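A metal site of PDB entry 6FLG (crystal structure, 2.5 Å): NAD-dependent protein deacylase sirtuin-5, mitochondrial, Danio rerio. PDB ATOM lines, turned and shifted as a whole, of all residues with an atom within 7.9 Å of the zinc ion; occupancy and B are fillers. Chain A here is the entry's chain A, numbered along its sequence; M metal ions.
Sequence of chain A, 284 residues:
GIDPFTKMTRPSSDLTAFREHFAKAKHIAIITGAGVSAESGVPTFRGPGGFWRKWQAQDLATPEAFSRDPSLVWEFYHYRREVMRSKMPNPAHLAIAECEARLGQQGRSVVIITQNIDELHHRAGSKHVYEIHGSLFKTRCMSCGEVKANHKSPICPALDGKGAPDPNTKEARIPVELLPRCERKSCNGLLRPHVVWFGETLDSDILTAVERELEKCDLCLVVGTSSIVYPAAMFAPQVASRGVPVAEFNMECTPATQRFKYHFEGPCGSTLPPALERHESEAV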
ATOM      1  N   ARG A 140      13.817 -16.389 -19.156  1.00  0.00           N
ATOM      2  CA  ARG A 140      15.245 -16.624 -19.304  1.00  0.00           C
ATOM      3  C   ARG A 140      15.894 -15.329 -19.788  1.00  0.00           C
ATOM      4  O   ARG A 140      15.394 -14.671 -20.708  1.00  0.00           O
ATOM      5  CB  ARG A 140      15.542 -17.789 -20.265  1.00  0.00           C
ATOM      6  CG  ARG A 140      17.041 -17.982 -20.485  1.00  0.00           C
ATOM      7  CD  ARG A 140      17.415 -19.368 -20.956  1.00  0.00           C
ATOM      8  NE  ARG A 140      17.071 -19.611 -22.363  1.00  0.00           N
ATOM      9  CZ  ARG A 140      15.968 -20.210 -22.809  1.00  0.00           C
ATOM     10  NH1 ARG A 140      15.024 -20.668 -21.986  1.00  0.00           N
ATOM     11  NH2 ARG A 140      15.800 -20.364 -24.127  1.00  0.00           N
ATOM     12  N   CYS A 141      17.016 -14.974 -19.165  1.00  0.00           N
ATOM     13  CA  CYS A 141      17.793 -13.800 -19.532  1.00  0.00           C
ATOM     14  C   CYS A 141      18.663 -14.145 -20.727  1.00  0.00           C
ATOM     15  O   CYS A 141      19.264 -15.224 -20.766  1.00  0.00           O
ATOM     16  CB  CYS A 141      18.673 -13.347 -18.362  1.00  0.00           C
ATOM     17  SG  CYS A 141      19.766 -11.969 -18.716  1.00  0.00           S
ATOM     18  N   MET A 142      18.749 -13.224 -21.689  1.00  0.00           N
ATOM     19  CA  MET A 142      19.566 -13.427 -22.892  1.00  0.00           C
ATOM     20  C   MET A 142      21.072 -13.291 -22.620  1.00  0.00           C
ATOM     21  O   MET A 142      21.851 -13.998 -23.250  1.00  0.00           O
ATOM     22  CB  MET A 142      19.132 -12.464 -24.007  1.00  0.00           C
ATOM     23  CG  MET A 142      17.715 -12.694 -24.499  1.00  0.00           C
ATOM     24  SD  MET A 142      17.518 -14.304 -25.252  1.00  0.00           S
ATOM     25  CE  MET A 142      17.810 -13.907 -26.968  1.00  0.00           C
ATOM     26  N   SER A 143      21.472 -12.404 -21.708  1.00  0.00           N
ATOM     27  CA  SER A 143      22.875 -12.268 -21.302  1.00  0.00           C
ATOM     28  C   SER A 143      23.356 -13.446 -20.456  1.00  0.00           C
ATOM     29  O   SER A 143      24.067 -14.326 -20.946  1.00  0.00           O
ATOM     30  CB  SER A 143      23.130 -10.962 -20.541  1.00  0.00           C
ATOM     31  OG  SER A 143      23.364  -9.882 -21.406  1.00  0.00           O
ATOM     32  N   CYS A 144      22.943 -13.468 -19.190  1.00  0.00           N
ATOM     33  CA  CYS A 144      23.505 -14.372 -18.177  1.00  0.00           C
ATOM     34  C   CYS A 144      22.828 -15.750 -18.081  1.00  0.00           C
ATOM     35  O   CYS A 144      23.398 -16.661 -17.471  1.00  0.00           O
ATOM     36  CB  CYS A 144      23.486 -13.687 -16.813  1.00  0.00           C
ATOM     37  SG  CYS A 144      21.817 -13.486 -16.136  1.00  0.00           S
ATOM     38  N   GLY A 145      21.621 -15.887 -18.639  1.00  0.00           N
ATOM     39  CA  GLY A 145      20.932 -17.182 -18.704  1.00  0.00           C
ATOM     40  C   GLY A 145      20.123 -17.630 -17.488  1.00  0.00           C
ATOM     41  O   GLY A 145      19.617 -18.768 -17.482  1.00  0.00           O
ATOM     42  N   GLU A 146      19.984 -16.762 -16.481  1.00  0.00           N
ATOM     43  CA  GLU A 146      19.226 -17.072 -15.262  1.00  0.00           C
ATOM     44  C   GLU A 146      17.771 -17.295 -15.592  1.00  0.00           C
ATOM     45  O   GLU A 146      17.212 -16.620 -16.450  1.00  0.00           O
ATOM     46  CB  GLU A 146      19.311 -15.939 -14.226  1.00  0.00           C
ATOM     47  CG  GLU A 146      18.583 -16.185 -12.898  1.00  0.00           C
ATOM     48  CD  GLU A 146      18.549 -14.953 -12.013  1.00  0.00           C
ATOM     49  OE1 GLU A 146      18.022 -13.905 -12.453  1.00  0.00           O
ATOM     50  OE2 GLU A 146      19.038 -15.014 -10.860  1.00  0.00           O
ATOM     51  N   ARG A 181      13.624  -6.514 -18.410  1.00  0.00           N
ATOM     52  CA  ARG A 181      15.061  -6.656 -18.220  1.00  0.00           C
ATOM     53  C   ARG A 181      15.385  -7.444 -16.951  1.00  0.00           C
ATOM     54  O   ARG A 181      14.559  -7.620 -16.053  1.00  0.00           O
ATOM     55  CB  ARG A 181      15.746  -5.290 -18.150  1.00  0.00           C
ATOM     56  CG  ARG A 181      15.376  -4.282 -19.229  1.00  0.00           C
ATOM     57  CD  ARG A 181      15.600  -4.786 -20.657  1.00  0.00           C
ATOM     58  NE  ARG A 181      17.018  -4.933 -20.975  1.00  0.00           N
ATOM     59  CZ  ARG A 181      17.535  -5.051 -22.205  1.00  0.00           C
ATOM     60  NH1 ARG A 181      16.763  -5.030 -23.297  1.00  0.00           N
ATOM     61  NH2 ARG A 181      18.850  -5.164 -22.343  1.00  0.00           N
ATOM     62  N   CYS A 182      16.632  -7.884 -16.883  1.00  0.00           N
ATOM     63  CA  CYS A 182      17.126  -8.766 -15.844  1.00  0.00           C
ATOM     64  C   CYS A 182      17.390  -8.001 -14.554  1.00  0.00           C
ATOM     65  O   CYS A 182      18.240  -7.109 -14.529  1.00  0.00           O
ATOM     66  CB  CYS A 182      18.422  -9.386 -16.353  1.00  0.00           C
ATOM     67  SG  CYS A 182      19.149 -10.724 -15.399  1.00  0.00           S
ATOM     68  N   GLU A 183      16.682  -8.356 -13.478  1.00  0.00           N
ATOM     69  CA  GLU A 183      16.763  -7.601 -12.208  1.00  0.00           C
ATOM     70  C   GLU A 183      18.147  -7.622 -11.525  1.00  0.00           C
ATOM     71  O   GLU A 183      18.425  -6.739 -10.706  1.00  0.00           O
ATOM     72  CB  GLU A 183      15.686  -8.073 -11.209  1.00  0.00           C
ATOM     73  CG  GLU A 183      14.245  -7.668 -11.522  1.00  0.00           C
ATOM     74  CD  GLU A 183      13.251  -8.233 -10.513  1.00  0.00           C
ATOM     75  OE1 GLU A 183      12.255  -8.889 -10.920  1.00  0.00           O
ATOM     76  OE2 GLU A 183      13.452  -8.041  -9.283  1.00  0.00           O
ATOM     77  N   ARG A 184      18.985  -8.610 -11.842  1.00  0.00           N
ATOM     78  CA  ARG A 184      20.359  -8.658 -11.313  1.00  0.00           C
ATOM     79  C   ARG A 184      21.168  -7.535 -11.942  1.00  0.00           C
ATOM     80  O   ARG A 184      21.473  -7.558 -13.139  1.00  0.00           O
ATOM     81  CB  ARG A 184      21.014 -10.042 -11.479  1.00  0.00           C
ATOM     82  CG  ARG A 184      20.726 -10.976 -10.291  1.00  0.00           C
ATOM     83  CD  ARG A 184      21.196 -12.411 -10.479  1.00  0.00           C
ATOM     84  NE  ARG A 184      22.610 -12.506 -10.839  1.00  0.00           N
ATOM     85  CZ  ARG A 184      23.108 -12.615 -12.083  1.00  0.00           C
ATOM     86  NH1 ARG A 184      22.301 -12.652 -13.148  1.00  0.00           N
ATOM     87  NH2 ARG A 184      24.423 -12.688 -12.269  1.00  0.00           N
ATOM     88  N   LYS A 185      21.498  -6.551 -11.093  1.00  0.00           N
ATOM     89  CA  LYS A 185      21.779  -5.169 -11.517  1.00  0.00           C
ATOM     90  C   LYS A 185      22.963  -4.982 -12.481  1.00  0.00           C
ATOM     91  O   LYS A 185      22.873  -4.174 -13.413  1.00  0.00           O
ATOM     92  CB  LYS A 185      21.927  -4.246 -10.293  1.00  0.00           C
ATOM     93  CG  LYS A 185      23.136  -4.502  -9.399  1.00  0.00           C
ATOM     94  CD  LYS A 185      23.069  -3.682  -8.128  1.00  0.00           C
ATOM     95  CE  LYS A 185      24.294  -3.911  -7.260  1.00  0.00           C
ATOM     96  NZ  LYS A 185      24.383  -2.946  -6.129  1.00  0.00           N
ATOM     97  N   SER A 186      24.043  -5.736 -12.270  1.00  0.00           N
ATOM     98  CA  SER A 186      25.194  -5.661 -13.177  1.00  0.00           C
ATOM     99  C   SER A 186      24.923  -6.203 -14.593  1.00  0.00           C
ATOM    100  O   SER A 186      25.750  -6.008 -15.480  1.00  0.00           O
ATOM    101  CB  SER A 186      26.408  -6.388 -12.576  1.00  0.00           C
ATOM    102  OG  SER A 186      26.138  -7.761 -12.398  1.00  0.00           O
ATOM    103  N   CYS A 187      23.786  -6.888 -14.786  1.00  0.00           N
ATOM    104  CA  CYS A 187      23.440  -7.500 -16.074  1.00  0.00           C
ATOM    105  C   CYS A 187      22.579  -6.627 -16.990  1.00  0.00           C
ATOM    106  O   CYS A 187      22.995  -6.267 -18.090  1.00  0.00           O
ATOM    107  CB  CYS A 187      22.726  -8.831 -15.829  1.00  0.00           C
ATOM    108  SG  CYS A 187      22.343  -9.701 -17.357  1.00  0.00           S
ATOM    109  N   ASN A 188      21.356  -6.342 -16.535  1.00  0.00           N
ATOM    110  CA  ASN A 188      20.340  -5.647 -17.343  1.00  0.00           C
ATOM    111  C   ASN A 188      20.064  -6.255 -18.726  1.00  0.00           C
ATOM    112  O   ASN A 188      19.695  -5.538 -19.663  1.00  0.00           O
ATOM    113  CB  ASN A 188      20.681  -4.145 -17.468  1.00  0.00           C
ATOM    114  CG  ASN A 188      19.493  -3.306 -17.909  1.00  0.00           C
ATOM    115  OD1 ASN A 188      18.362  -3.516 -17.488  1.00  0.00           O
ATOM    116  ND2 ASN A 188      19.754  -2.335 -18.769  1.00  0.00           N
ATOM    117  N   GLY A 189      20.206  -7.576 -18.849  1.00  0.00           N
ATOM    118  CA  GLY A 189      19.922  -8.261 -20.098  1.00  0.00           C
ATOM    119  C   GLY A 189      18.437  -8.285 -20.453  1.00  0.00           C
ATOM    120  O   GLY A 189      17.581  -8.262 -19.579  1.00  0.00           O
ATOM    121  N   LEU A 190      18.146  -8.334 -21.750  1.00  0.00           N
ATOM    122  CA  LEU A 190      16.784  -8.532 -22.252  1.00  0.00           C
ATOM    123  C   LEU A 190      16.317  -9.909 -21.864  1.00  0.00           C
ATOM    124  O   LEU A 190      17.047 -10.884 -22.076  1.00  0.00           O
ATOM    125  CB  LEU A 190      16.765  -8.436 -23.781  1.00  0.00           C
ATOM    126  CG  LEU A 190      15.458  -8.726 -24.514  1.00  0.00           C
ATOM    127  CD1 LEU A 190      14.406  -7.707 -24.119  1.00  0.00           C
ATOM    128  CD2 LEU A 190      15.653  -8.740 -26.023  1.00  0.00           C
ATOM    129  N   LEU A 191      15.121 -10.022 -21.298  1.00  0.00           N
ATOM    130  CA  LEU A 191      14.555 -11.326 -20.973  1.00  0.00           C
ATOM    131  C   LEU A 191      13.694 -11.827 -22.117  1.00  0.00           C
ATOM    132  O   LEU A 191      13.324 -11.073 -23.008  1.00  0.00           O
ATOM    133  CB  LEU A 191      13.732 -11.269 -19.691  1.00  0.00           C
ATOM    134  CG  LEU A 191      14.392 -10.642 -18.456  1.00  0.00           C
ATOM    135  CD1 LEU A 191      13.453 -10.747 -17.274  1.00  0.00           C
ATOM    136  CD2 LEU A 191      15.725 -11.296 -18.159  1.00  0.00           C
HETATM  137 ZN    ZN M   1      20.907 -11.415 -16.764  1.00  0.00          ZN
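The side-chain sulfur (SG) of Cys 144 lies close to the backbone NH (N) of Glu 146 (3.8 Å). The backbone NH of Cys 182 sits at hydrogen-bond distance from the backbone carbonyl oxygen of Gly 189 (2.9 Å). The side-chain sulfur of Cys 187 sits close to the backbone NH of Gly 189, 3.4 Å away. N of Ser 143 lies close to SG of Cys 141, at 3.5 Å. SG of Cys 144 lies close to NH1 of Arg 184 (3.1 Å). The backbone carbonyl oxygen (O) of Glu 146 is in hydrogen-bond range of the backbone NH (N) of Cys 141 (3.2 Å).
Of the 18 residues printed, 4 come within 4 Å of the zinc ion.
The side-chain sulfur (SG) of Cys 187 binds the zinc ion (2.3 Å). SG of Cys 141 is bound to the zinc ion, at 2.3 Å. SG of Cys 182 binds the zinc ion (2.3 Å). The zinc ion is bound by SG of Cys 144, 2.3 Å away. The zinc ion has four donor atoms within binding distance.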
